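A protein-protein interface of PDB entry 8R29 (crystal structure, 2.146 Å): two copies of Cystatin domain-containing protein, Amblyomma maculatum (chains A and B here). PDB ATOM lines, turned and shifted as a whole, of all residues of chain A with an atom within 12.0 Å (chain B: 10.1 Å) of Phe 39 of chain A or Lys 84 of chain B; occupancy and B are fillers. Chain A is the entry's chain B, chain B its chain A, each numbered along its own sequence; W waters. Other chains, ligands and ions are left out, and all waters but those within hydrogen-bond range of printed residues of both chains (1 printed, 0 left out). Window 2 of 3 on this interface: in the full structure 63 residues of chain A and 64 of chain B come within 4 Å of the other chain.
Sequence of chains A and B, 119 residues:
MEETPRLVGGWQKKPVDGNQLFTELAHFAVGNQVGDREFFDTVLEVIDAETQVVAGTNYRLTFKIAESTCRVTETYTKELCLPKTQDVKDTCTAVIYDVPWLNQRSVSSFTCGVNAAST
N of Thr 42 of chain A lies within hydrogen-bond range of O of Ala 66 of chain B (3.0 Å). O of Phe 40 of chain A sits at hydrogen-bond distance from OG of Ser 68 of chain B, at 2.6 Å. The backbone NH (N) of Phe 40 of chain A sits at hydrogen-bond distance from the backbone carbonyl oxygen (O) of Cys 70 of chain B (2.8 Å). The backbone NH of Val 72 of chain B sits at hydrogen-bond distance from the backbone carbonyl oxygen of Glu 38 of chain A (2.8 Å). A ring nitrogen (ND1) of His 27 of chain A is in hydrogen-bond range of the side-chain hydroxyl of Tyr 76 of chain B, at 2.5 Å. The side-chain hydroxyl of Tyr 76 of chain B lies within hydrogen-bond range of the side-chain hydroxyl of Thr 42 of chain A (2.9 Å). O of Cys 81 of chain B is in hydrogen-bond range of OG1 of Thr 42 of chain A, 3.1 Å away. The side-chain carboxylate of Asp 41 of chain A is in salt-bridge range of the side-chain amino group of Lys 89 of chain B, at 2.8 Å.
The side-chain carboxylate (OE2) of Glu 67 of chain B lies within salt-bridge range of the side-chain amino group (NZ) of Lys 84 of chain B (2.8 Å). The backbone NH (N) of Thr 69 of chain B sits at hydrogen-bond distance from the backbone carbonyl oxygen (O) of Leu 82 of chain B (3.2 Å). SG of Cys 81 of chain B is disulfide-bonded to SG of Cys 70 of chain B, at 2.2 Å. NE of Arg 37 of chain A sits at hydrogen-bond distance from O of Gln 33 of chain A (3.1 Å).
Among the printed residues, pairs that only touch across the chains: Phe 39 of chain A with Cys 70 of chain B, Asp 41 of chain A with Ala 66 of chain B, Thr 42 of chain A with Ile 65 of chain B, Glu 38 of chain A with Arg 71 of chain B, Phe 39 of chain A with Thr 69 of chain B, Phe 39 of chain A with Glu 67 of chain B, Phe 40 of chain A with Glu 74 of chain B, Phe 39 of chain A with Ser 68 of chain B, Leu 44 of chain A with Ile 65 of chain B, Gly 31 of chain A with Tyr 76 of chain B, Phe 39 of chain A with Lys 84 of chain B, Asp 41 of chain A with Tyr 76 of chain B, Phe 40 of chain A with Val 72 of chain B, Asp 41 of chain A with Glu 67 of chain B, Phe 39 of chain A with Arg 71 of chain B, Arg 37 of chain A with Val 72 of chain B, Phe 39 of chain A with Val 72 of chain B, Phe 40 of chain A with Tyr 76 of chain B, Val 30 of chain A with Tyr 76 of chain B, Leu 44 of chain A with Ala 66 of chain B, Phe 40 of chain A with Arg 71 of chain B, Asp 41 of chain A with Ile 65 of chain B, Thr 42 of chain A with Pro 83 of chain B, Thr 42 of chain A with Ser 68 of chain B, Leu 44 of chain A with Val 88 of chain B, Leu 44 of chain A with Pro 83 of chain B and Phe 40 of chain A with Glu 67 of chain B.
Of the printed residues of chain B, Gly 31 of chain A touches Tyr 76. Of chain B, only Arg 71 and Val 72 come within 4 Å of Glu 38 of chain A. Printed residues of chain B within 4 Å of Asp 41 of chain A: Ile 65 (3.8 Å), Ala 66 (3.2 Å), Glu 67 (3.5 Å), Tyr 76 (3.5 Å) and Lys 89 (2.8 Å). Of the printed residues of chain A, Ile 65 of chain B touches Asp 41 (3.8 Å), Thr 42 (3.3 Å) and Leu 44 (3.5 Å). Of chain A, only Phe 39 (3.3 Å) comes within 4 Å of Thr 69 of chain B. Cys 70 of chain B touches two residues of chain A. Arg 71 of chain B touches just these residues of chain A: Glu 38 (3.3 Å), Phe 39 (3.6 Å) and Phe 40 (3.7 Å). Val 72 of chain B touches just these residues of chain A: Arg 37, Glu 38, Phe 39 and Phe 40. Of the printed residues of chain A, Glu 74 of chain B touches Phe 40 (3.3 Å). Leu 80 of chain B touches none of the printed residues of chain A. Of chain A, only Phe 39 comes within 4 Å of Lys 84 of chain B. Gln 86 of chain B touches none of the printed residues of chain A. The nearest residue of chain A that does not touch Lys 84 of chain B is Thr 42 of chain A (5.9 Å). The nearest printed residue of chain B that does not touch His 27 of chain A is Cys 81 of chain B (5.6 Å).
Of the 17 printed residues of chain A, 10 touch a printed residue of chain B. Printed residues of chain A that touch a printed residue of chain B: His 27, Val 30, Gly 31, Arg 37, Glu 38, Phe 39, Phe 40, Asp 41, Thr 42 and Leu 44. Hydrophobic or aromatic side chains of chain A within 4 Å of the printed part of chain B: His 27, Val 30, Phe 39, Phe 40 and Leu 44. Of the 21 printed residues of chain B, 15 touch a printed residue of chain A. Printed residues of chain B that touch a printed residue of chain A: Ile 65, Ala 66, Glu 67, Ser 68, Thr 69, Cys 70, Arg 71, Val 72, Glu 74, Tyr 76, Cys 81, Pro 83, Lys 84, Val 88 and Lys 89. Hydrophobic or aromatic side chains of chain B within 4 Å of the printed part of chain A: Ile 65, Ala 66, Val 72, Tyr 76 and Pro 83. Among the printed residues, Asp or Glu carboxylates within 4 Å of a Lys or Arg side-chain nitrogen of the other chain: Asp 41 of chain A with Lys 89 of chain B (2.8 Å).
No position is printed for both chains.
Water W1 bridges the side-chain hydroxyl (OG1) of Thr 42 of chain A and the backbone carbonyl oxygen (O) of Cys 81 of chain B.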
ATOM      1  N   HIS A  27       8.790  30.488  18.423  1.00  0.00           N
ATOM      2  CA  HIS A  27       9.213  30.101  19.772  1.00  0.00           C
ATOM      3  C   HIS A  27       8.940  28.629  20.016  1.00  0.00           C
ATOM      4  O   HIS A  27       9.763  27.938  20.590  1.00  0.00           O
ATOM      5  CB  HIS A  27       8.490  30.951  20.829  1.00  0.00           C
ATOM      6  CG  HIS A  27       9.186  32.273  21.082  1.00  0.00           C
ATOM      7  ND1 HIS A  27      10.478  32.351  21.574  1.00  0.00           N
ATOM      8  CD2 HIS A  27       8.758  33.527  20.920  1.00  0.00           C
ATOM      9  CE1 HIS A  27      10.814  33.621  21.700  1.00  0.00           C
ATOM     10  NE2 HIS A  27       9.758  34.362  21.339  1.00  0.00           N
ATOM     11  N   ALA A  29       8.672  26.172  17.732  1.00  0.00           N
ATOM     12  CA  ALA A  29       9.680  25.372  17.030  1.00  0.00           C
ATOM     13  C   ALA A  29      11.052  25.416  17.742  1.00  0.00           C
ATOM     14  O   ALA A  29      11.654  24.366  17.952  1.00  0.00           O
ATOM     15  CB  ALA A  29       9.803  25.856  15.606  1.00  0.00           C
ATOM     16  N   VAL A  30      11.588  26.595  18.050  1.00  0.00           N
ATOM     17  CA  VAL A  30      12.948  26.692  18.610  1.00  0.00           C
ATOM     18  C   VAL A  30      13.002  26.032  19.978  1.00  0.00           C
ATOM     19  O   VAL A  30      13.915  25.283  20.228  1.00  0.00           O
ATOM     20  CB  VAL A  30      13.515  28.129  18.678  1.00  0.00           C
ATOM     21  CG1 VAL A  30      13.087  28.901  19.915  1.00  0.00           C
ATOM     22  CG2 VAL A  30      15.008  28.112  18.666  1.00  0.00           C
ATOM     23  N   GLY A  31      11.970  26.208  20.804  1.00  0.00           N
ATOM     24  CA  GLY A  31      11.932  25.590  22.129  1.00  0.00           C
ATOM     25  C   GLY A  31      11.828  24.070  22.135  1.00  0.00           C
ATOM     26  O   GLY A  31      11.802  23.450  23.216  1.00  0.00           O
ATOM     27  N   ASN A  32      11.663  23.456  20.948  1.00  0.00           N
ATOM     28  CA  ASN A  32      11.569  21.995  20.879  1.00  0.00           C
ATOM     29  C   ASN A  32      12.842  21.435  20.220  1.00  0.00           C
ATOM     30  O   ASN A  32      12.853  20.287  19.847  1.00  0.00           O
ATOM     31  CB  ASN A  32      10.277  21.502  20.200  1.00  0.00           C
ATOM     32  CG  ASN A  32       9.059  21.600  21.100  1.00  0.00           C
ATOM     33  OD1 ASN A  32       8.962  20.942  22.130  1.00  0.00           O
ATOM     34  ND2 ASN A  32       8.103  22.457  20.784  1.00  0.00           N
ATOM     35  N   GLN A  33      13.909  22.244  20.069  1.00  0.00           N
ATOM     36  CA  GLN A  33      15.199  21.781  19.568  1.00  0.00           C
ATOM     37  C   GLN A  33      16.230  21.688  20.706  1.00  0.00           C
ATOM     38  O   GLN A  33      16.876  22.660  21.079  1.00  0.00           O
ATOM     39  CB  GLN A  33      15.764  22.724  18.494  1.00  0.00           C
ATOM     40  CG  GLN A  33      14.760  23.169  17.429  1.00  0.00           C
ATOM     41  CD  GLN A  33      14.116  22.019  16.693  1.00  0.00           C
ATOM     42  OE1 GLN A  33      14.807  21.184  16.106  1.00  0.00           O
ATOM     43  NE2 GLN A  33      12.784  21.980  16.708  1.00  0.00           N
ATOM     44  N   VAL A  34      16.463  20.479  21.204  1.00  0.00           N
ATOM     45  CA  VAL A  34      17.371  20.248  22.324  1.00  0.00           C
ATOM     46  C   VAL A  34      18.682  19.587  21.881  1.00  0.00           C
ATOM     47  O   VAL A  34      19.465  19.185  22.733  1.00  0.00           O
ATOM     48  CB  VAL A  34      16.663  19.385  23.387  1.00  0.00           C
ATOM     49  CG1 VAL A  34      15.343  20.012  23.799  1.00  0.00           C
ATOM     50  CG2 VAL A  34      16.466  17.948  22.912  1.00  0.00           C
ATOM     51  N   GLY A  35      18.914  19.418  20.575  1.00  0.00           N
ATOM     52  CA  GLY A  35      20.084  18.696  20.081  1.00  0.00           C
ATOM     53  C   GLY A  35      21.356  19.547  20.071  1.00  0.00           C
ATOM     54  O   GLY A  35      21.319  20.706  19.647  1.00  0.00           O
ATOM     55  N   ASP A  36      22.468  18.982  20.581  1.00  0.00           N
ATOM     56  CA  ASP A  36      23.830  19.510  20.411  1.00  0.00           C
ATOM     57  C   ASP A  36      24.003  20.863  21.119  1.00  0.00           C
ATOM     58  O   ASP A  36      24.707  21.753  20.635  1.00  0.00           O
ATOM     59  CB  ASP A  36      24.244  19.595  18.930  1.00  0.00           C
ATOM     60  N   ARG A  37      23.384  20.998  22.295  1.00  0.00           N
ATOM     61  CA  ARG A  37      23.136  22.293  22.899  1.00  0.00           C
ATOM     62  C   ARG A  37      22.959  22.108  24.397  1.00  0.00           C
ATOM     63  O   ARG A  37      22.220  21.213  24.819  1.00  0.00           O
ATOM     64  CB  ARG A  37      21.829  22.898  22.369  1.00  0.00           C
ATOM     65  CG  ARG A  37      21.964  23.737  21.107  1.00  0.00           C
ATOM     66  CD  ARG A  37      20.668  24.446  20.798  1.00  0.00           C
ATOM     67  NE  ARG A  37      19.745  23.480  20.245  1.00  0.00           N
ATOM     68  CZ  ARG A  37      19.428  23.362  18.956  1.00  0.00           C
ATOM     69  NH1 ARG A  37      19.067  22.169  18.528  1.00  0.00           N
ATOM     70  NH2 ARG A  37      19.540  24.371  18.101  1.00  0.00           N
ATOM     71  N   GLU A  38      23.603  22.980  25.182  1.00  0.00           N
ATOM     72  CA  GLU A  38      23.432  22.951  26.622  1.00  0.00           C
ATOM     73  C   GLU A  38      22.228  23.830  26.945  1.00  0.00           C
ATOM     74  O   GLU A  38      21.437  23.515  27.842  1.00  0.00           O
ATOM     75  CB  GLU A  38      24.720  23.397  27.328  1.00  0.00           C
ATOM     76  N   PHE A  39      22.099  24.937  26.194  1.00  0.00           N
ATOM     77  CA  PHE A  39      21.019  25.885  26.426  1.00  0.00           C
ATOM     78  C   PHE A  39      20.155  25.982  25.174  1.00  0.00           C
ATOM     79  O   PHE A  39      20.661  25.997  24.042  1.00  0.00           O
ATOM     80  CB  PHE A  39      21.563  27.265  26.770  1.00  0.00           C
ATOM     81  CG  PHE A  39      22.437  27.330  28.006  1.00  0.00           C
ATOM     82  CD1 PHE A  39      23.735  26.834  27.988  1.00  0.00           C
ATOM     83  CD2 PHE A  39      21.961  27.881  29.184  1.00  0.00           C
ATOM     84  CE1 PHE A  39      24.542  26.914  29.107  1.00  0.00           C
ATOM     85  CE2 PHE A  39      22.770  27.951  30.300  1.00  0.00           C
ATOM     86  CZ  PHE A  39      24.054  27.464  30.264  1.00  0.00           C
ATOM     87  N   PHE A  40      18.848  26.085  25.389  1.00  0.00           N
ATOM     88  CA  PHE A  40      17.935  26.408  24.312  1.00  0.00           C
ATOM     89  C   PHE A  40      18.351  27.701  23.634  1.00  0.00           C
ATOM     90  O   PHE A  40      18.791  28.628  24.305  1.00  0.00           O
ATOM     91  CB  PHE A  40      16.523  26.645  24.819  1.00  0.00           C
ATOM     92  CG  PHE A  40      15.769  25.436  25.280  1.00  0.00           C
ATOM     93  CD1 PHE A  40      15.419  24.433  24.376  1.00  0.00           C
ATOM     94  CD2 PHE A  40      15.294  25.357  26.574  1.00  0.00           C
ATOM     95  CE1 PHE A  40      14.673  23.345  24.793  1.00  0.00           C
ATOM     96  CE2 PHE A  40      14.517  24.276  26.979  1.00  0.00           C
ATOM     97  CZ  PHE A  40      14.222  23.274  26.088  1.00  0.00           C
ATOM     98  N   ASP A  41      18.189  27.721  22.307  1.00  0.00           N
ATOM     99  CA  ASP A  41      18.102  28.948  21.544  1.00  0.00           C
ATOM    100  C   ASP A  41      16.690  29.542  21.664  1.00  0.00           C
ATOM    101  O   ASP A  41      15.745  28.852  22.006  1.00  0.00           O
ATOM    102  CB  ASP A  41      18.524  28.690  20.096  1.00  0.00           C
ATOM    103  CG  ASP A  41      19.914  28.081  19.962  1.00  0.00           C
ATOM    104  OD1 ASP A  41      20.846  28.538  20.690  1.00  0.00           O
ATOM    105  OD2 ASP A  41      20.070  27.170  19.110  1.00  0.00           O
ATOM    106  N   THR A  42      16.576  30.843  21.402  1.00  0.00           N
ATOM    107  CA  THR A  42      15.325  31.573  21.458  1.00  0.00           C
ATOM    108  C   THR A  42      15.269  32.465  20.227  1.00  0.00           C
ATOM    109  O   THR A  42      16.268  32.654  19.554  1.00  0.00           O
ATOM    110  CB  THR A  42      15.264  32.402  22.732  1.00  0.00           C
ATOM    111  OG1 THR A  42      13.936  32.890  22.880  1.00  0.00           O
ATOM    112  CG2 THR A  42      16.257  33.550  22.743  1.00  0.00           C
ATOM    113  N   VAL A  43      14.113  33.051  19.981  1.00  0.00           N
ATOM    114  CA  VAL A  43      13.826  33.730  18.740  1.00  0.00           C
ATOM    115  C   VAL A  43      14.086  35.204  18.986  1.00  0.00           C
ATOM    116  O   VAL A  43      13.514  35.754  19.927  1.00  0.00           O
ATOM    117  CB  VAL A  43      12.343  33.532  18.331  1.00  0.00           C
ATOM    118  CG1 VAL A  43      11.985  34.330  17.099  1.00  0.00           C
ATOM    119  CG2 VAL A  43      11.963  32.101  18.155  1.00  0.00           C
ATOM    120  N   LEU A  44      14.852  35.828  18.081  1.00  0.00           N
ATOM    121  CA  LEU A  44      15.085  37.265  18.106  1.00  0.00           C
ATOM    122  C   LEU A  44      14.036  38.011  17.292  1.00  0.00           C
ATOM    123  O   LEU A  44      13.406  38.923  17.781  1.00  0.00           O
ATOM    124  CB  LEU A  44      16.476  37.523  17.541  1.00  0.00           C
ATOM    125  CG  LEU A  44      17.625  37.263  18.498  1.00  0.00           C
ATOM    126  CD1 LEU A  44      18.962  37.453  17.787  1.00  0.00           C
ATOM    127  CD2 LEU A  44      17.499  38.187  19.703  1.00  0.00           C
ATOM    128  N   ILE B  65      17.777  33.722  15.446  1.00  0.00           N
ATOM    129  CA  ILE B  65      17.907  33.142  16.778  1.00  0.00           C
ATOM    130  C   ILE B  65      19.121  33.695  17.523  1.00  0.00           C
ATOM    131  O   ILE B  65      20.019  34.277  16.915  1.00  0.00           O
ATOM    132  CB  ILE B  65      17.959  31.613  16.701  1.00  0.00           C
ATOM    133  CG1 ILE B  65      19.226  31.098  16.038  1.00  0.00           C
ATOM    134  CG2 ILE B  65      16.712  31.086  16.027  1.00  0.00           C
ATOM    135  CD1 ILE B  65      19.436  29.622  16.293  1.00  0.00           C
ATOM    136  N   ALA B  66      19.097  33.524  18.856  1.00  0.00           N
ATOM    137  CA  ALA B  66      20.200  33.799  19.760  1.00  0.00           C
ATOM    138  C   ALA B  66      20.283  32.640  20.746  1.00  0.00           C
ATOM    139  O   ALA B  66      19.348  31.852  20.845  1.00  0.00           O
ATOM    140  CB  ALA B  66      19.936  35.093  20.484  1.00  0.00           C
ATOM    141  N   GLU B  67      21.402  32.493  21.459  1.00  0.00           N
ATOM    142  CA  GLU B  67      21.456  31.506  22.524  1.00  0.00           C
ATOM    143  C   GLU B  67      20.667  32.099  23.671  1.00  0.00           C
ATOM    144  O   GLU B  67      20.773  33.298  23.924  1.00  0.00           O
ATOM    145  CB  GLU B  67      22.876  31.188  22.986  1.00  0.00           C
ATOM    146  CG  GLU B  67      22.948  30.222  24.167  1.00  0.00           C
ATOM    147  CD  GLU B  67      24.327  29.762  24.618  1.00  0.00           C
ATOM    148  OE1 GLU B  67      25.328  30.309  24.145  1.00  0.00           O
ATOM    149  OE2 GLU B  67      24.393  28.842  25.459  1.00  0.00           O
ATOM    150  N   SER B  68      19.862  31.256  24.319  1.00  0.00           N
ATOM    151  CA  SER B  68      19.065  31.683  25.446  1.00  0.00           C
ATOM    152  C   SER B  68      19.825  31.315  26.723  1.00  0.00           C
ATOM    153  O   SER B  68      20.777  30.532  26.643  1.00  0.00           O
ATOM    154  CB  SER B  68      17.690  31.038  25.408  1.00  0.00           C
ATOM    155  OG  SER B  68      17.630  29.912  26.306  1.00  0.00           O
ATOM    156  N   THR B  69      19.314  31.825  27.862  1.00  0.00           N
ATOM    157  CA  THR B  69      19.831  31.572  29.195  1.00  0.00           C
ATOM    158  C   THR B  69      19.322  30.257  29.779  1.00  0.00           C
ATOM    159  O   THR B  69      19.863  29.823  30.807  1.00  0.00           O
ATOM    160  CB  THR B  69      19.442  32.706  30.155  1.00  0.00           C
ATOM    161  OG1 THR B  69      18.014  32.735  30.309  1.00  0.00           O
ATOM    162  CG2 THR B  69      19.922  34.070  29.701  1.00  0.00           C
ATOM    163  N   CYS B  70      18.289  29.635  29.169  1.00  0.00           N
ATOM    164  CA  CYS B  70      17.725  28.408  29.720  1.00  0.00           C
ATOM    165  C   CYS B  70      18.485  27.164  29.232  1.00  0.00           C
ATOM    166  O   CYS B  70      18.647  26.952  28.040  1.00  0.00           O
ATOM    167  CB  CYS B  70      16.256  28.205  29.351  1.00  0.00           C
ATOM    168  SG  CYS B  70      15.091  29.420  30.033  1.00  0.00           S
ATOM    169  N   ARG B  71      18.888  26.324  30.186  1.00  0.00           N
ATOM    170  CA  ARG B  71      19.426  24.994  29.946  1.00  0.00           C
ATOM    171  C   ARG B  71      18.328  24.086  29.358  1.00  0.00           C
ATOM    172  O   ARG B  71      17.122  24.229  29.669  1.00  0.00           O
ATOM    173  CB  ARG B  71      20.056  24.471  31.254  1.00  0.00           C
ATOM    174  N   VAL B  72      18.750  23.147  28.493  1.00  0.00           N
ATOM    175  CA  VAL B  72      17.774  22.312  27.801  1.00  0.00           C
ATOM    176  C   VAL B  72      17.085  21.345  28.772  1.00  0.00           C
ATOM    177  O   VAL B  72      16.070  20.775  28.421  1.00  0.00           O
ATOM    178  CB  VAL B  72      18.369  21.577  26.591  1.00  0.00           C
ATOM    179  CG1 VAL B  72      18.927  22.551  25.555  1.00  0.00           C
ATOM    180  CG2 VAL B  72      19.411  20.554  27.020  1.00  0.00           C
ATOM    181  N   THR B  73      17.567  21.216  30.014  1.00  0.00           N
ATOM    182  CA  THR B  73      16.901  20.383  31.010  1.00  0.00           C
ATOM    183  C   THR B  73      15.559  21.006  31.419  1.00  0.00           C
ATOM    184  O   THR B  73      14.677  20.315  31.931  1.00  0.00           O
ATOM    185  CB  THR B  73      17.803  20.144  32.233  1.00  0.00           C
ATOM    186  OG1 THR B  73      17.954  21.369  32.957  1.00  0.00           O
ATOM    187  CG2 THR B  73      19.170  19.600  31.877  1.00  0.00           C
ATOM    188  N   GLU B  74      15.447  22.325  31.233  1.00  0.00           N
ATOM    189  CA  GLU B  74      14.304  23.103  31.690  1.00  0.00           C
ATOM    190  C   GLU B  74      13.185  23.006  30.648  1.00  0.00           C
ATOM    191  O   GLU B  74      13.413  22.505  29.557  1.00  0.00           O
ATOM    192  CB  GLU B  74      14.702  24.564  31.956  1.00  0.00           C
ATOM    193  N   TYR B  76      10.985  25.191  28.189  1.00  0.00           N
ATOM    194  CA  TYR B  76      11.191  26.420  27.472  1.00  0.00           C
ATOM    195  C   TYR B  76       9.953  27.281  27.617  1.00  0.00           C
ATOM    196  O   TYR B  76       8.864  26.746  27.618  1.00  0.00           O
ATOM    197  CB  TYR B  76      11.472  26.101  26.005  1.00  0.00           C
ATOM    198  CG  TYR B  76      11.621  27.323  25.125  1.00  0.00           C
ATOM    199  CD1 TYR B  76      10.501  27.973  24.628  1.00  0.00           C
ATOM    200  CD2 TYR B  76      12.865  27.903  24.908  1.00  0.00           C
ATOM    201  CE1 TYR B  76      10.639  29.087  23.817  1.00  0.00           C
ATOM    202  CE2 TYR B  76      13.015  29.050  24.156  1.00  0.00           C
ATOM    203  CZ  TYR B  76      11.898  29.631  23.588  1.00  0.00           C
ATOM    204  OH  TYR B  76      11.961  30.800  22.890  1.00  0.00           O
ATOM    205  N   LEU B  80      10.672  33.212  29.990  1.00  0.00           N
ATOM    206  CA  LEU B  80      11.796  32.846  30.840  1.00  0.00           C
ATOM    207  C   LEU B  80      13.107  32.760  30.067  1.00  0.00           C
ATOM    208  O   LEU B  80      14.169  33.076  30.620  1.00  0.00           O
ATOM    209  CB  LEU B  80      11.512  31.528  31.566  1.00  0.00           C
ATOM    210  CG  LEU B  80      10.234  31.508  32.403  1.00  0.00           C
ATOM    211  CD1 LEU B  80      10.175  30.268  33.298  1.00  0.00           C
ATOM    212  CD2 LEU B  80      10.070  32.775  33.230  1.00  0.00           C
ATOM    213  N   CYS B  81      13.059  32.324  28.806  1.00  0.00           N
ATOM    214  CA  CYS B  81      14.275  31.969  28.080  1.00  0.00           C
ATOM    215  C   CYS B  81      14.647  33.132  27.153  1.00  0.00           C
ATOM    216  O   CYS B  81      14.462  33.057  25.932  1.00  0.00           O
ATOM    217  CB  CYS B  81      14.097  30.648  27.330  1.00  0.00           C
ATOM    218  SG  CYS B  81      13.609  29.257  28.397  1.00  0.00           S
ATOM    219  N   LEU B  82      15.116  34.227  27.781  1.00  0.00           N
ATOM    220  CA  LEU B  82      15.523  35.439  27.088  1.00  0.00           C
ATOM    221  C   LEU B  82      16.916  35.251  26.503  1.00  0.00           C
ATOM    222  O   LEU B  82      17.644  34.364  26.938  1.00  0.00           O
ATOM    223  CB  LEU B  82      15.449  36.620  28.058  1.00  0.00           C
ATOM    224  CG  LEU B  82      14.057  36.823  28.671  1.00  0.00           C
ATOM    225  CD1 LEU B  82      14.033  38.054  29.556  1.00  0.00           C
ATOM    226  CD2 LEU B  82      12.983  36.964  27.603  1.00  0.00           C
ATOM    227  N   PRO B  83      17.290  36.022  25.448  1.00  0.00           N
ATOM    228  CA  PRO B  83      18.611  35.926  24.815  1.00  0.00           C
ATOM    229  C   PRO B  83      19.734  36.299  25.794  1.00  0.00           C
ATOM    230  O   PRO B  83      19.547  37.193  26.622  1.00  0.00           O
ATOM    231  CB  PRO B  83      18.542  36.976  23.713  1.00  0.00           C
ATOM    232  CG  PRO B  83      17.064  37.308  23.510  1.00  0.00           C
ATOM    233  CD  PRO B  83      16.455  37.081  24.863  1.00  0.00           C
ATOM    234  N   LYS B  84      20.849  35.561  25.820  1.00  0.00           N
ATOM    235  CA  LYS B  84      21.977  35.969  26.667  1.00  0.00           C
ATOM    236  C   LYS B  84      22.422  37.366  26.238  1.00  0.00           C
ATOM    237  O   LYS B  84      22.446  38.299  27.046  1.00  0.00           O
ATOM    238  CB  LYS B  84      23.169  35.003  26.623  1.00  0.00           C
ATOM    239  CG  LYS B  84      23.067  33.852  27.598  1.00  0.00           C
ATOM    240  CD  LYS B  84      23.929  32.654  27.296  1.00  0.00           C
ATOM    241  CE  LYS B  84      23.563  31.504  28.204  1.00  0.00           C
ATOM    242  NZ  LYS B  84      24.284  30.275  27.841  1.00  0.00           N
ATOM    243  N   THR B  85      22.707  37.475  24.936  1.00  0.00           N
ATOM    244  CA  THR B  85      23.188  38.682  24.296  1.00  0.00           C
ATOM    245  C   THR B  85      22.302  38.931  23.079  1.00  0.00           C
ATOM    246  O   THR B  85      21.821  37.975  22.482  1.00  0.00           O
ATOM    247  CB  THR B  85      24.676  38.519  23.936  1.00  0.00           C
ATOM    248  OG1 THR B  85      25.104  39.671  23.214  1.00  0.00           O
ATOM    249  CG2 THR B  85      24.984  37.309  23.084  1.00  0.00           C
ATOM    250  N   GLN B  86      22.152  40.198  22.676  1.00  0.00           N
ATOM    251  CA  GLN B  86      21.435  40.534  21.464  1.00  0.00           C
ATOM    252  C   GLN B  86      22.229  40.147  20.214  1.00  0.00           C
ATOM    253  O   GLN B  86      21.855  40.580  19.136  1.00  0.00           O
ATOM    254  CB  GLN B  86      21.091  42.027  21.485  1.00  0.00           C
ATOM    255  N   ASP B  87      23.253  39.282  20.330  1.00  0.00           N
ATOM    256  CA  ASP B  87      23.996  38.790  19.174  1.00  0.00           C
ATOM    257  C   ASP B  87      23.225  37.701  18.427  1.00  0.00           C
ATOM    258  O   ASP B  87      22.993  36.605  18.955  1.00  0.00           O
ATOM    259  CB  ASP B  87      25.342  38.145  19.535  1.00  0.00           C
ATOM    260  CG  ASP B  87      26.474  39.089  19.917  1.00  0.00           C
ATOM    261  OD1 ASP B  87      26.334  40.338  19.721  1.00  0.00           O
ATOM    262  OD2 ASP B  87      27.487  38.560  20.417  1.00  0.00           O
ATOM    263  N   VAL B  88      22.951  37.962  17.148  1.00  0.00           N
ATOM    264  CA  VAL B  88      22.471  36.930  16.240  1.00  0.00           C
ATOM    265  C   VAL B  88      23.431  35.747  16.240  1.00  0.00           C
ATOM    266  O   VAL B  88      24.639  35.919  16.218  1.00  0.00           O
ATOM    267  CB  VAL B  88      22.312  37.462  14.807  1.00  0.00           C
ATOM    268  CG1 VAL B  88      21.899  36.354  13.862  1.00  0.00           C
ATOM    269  CG2 VAL B  88      21.358  38.645  14.729  1.00  0.00           C
ATOM    270  N   LYS B  89      22.882  34.540  16.264  1.00  0.00           N
ATOM    271  CA  LYS B  89      23.704  33.348  16.194  1.00  0.00           C
ATOM    272  C   LYS B  89      23.507  32.708  14.834  1.00  0.00           C
ATOM    273  O   LYS B  89      24.472  32.322  14.195  1.00  0.00           O
ATOM    274  CB  LYS B  89      23.346  32.304  17.262  1.00  0.00           C
ATOM    275  CG  LYS B  89      24.087  30.989  17.096  1.00  0.00           C
ATOM    276  CD  LYS B  89      23.438  29.804  17.707  1.00  0.00           C
ATOM    277  CE  LYS B  89      23.625  29.720  19.196  1.00  0.00           C
ATOM    278  NZ  LYS B  89      23.412  28.312  19.623  1.00  0.00           N
HETATM  279  O   HOH W   1      12.772  34.649  24.528  1.00  0.00           O
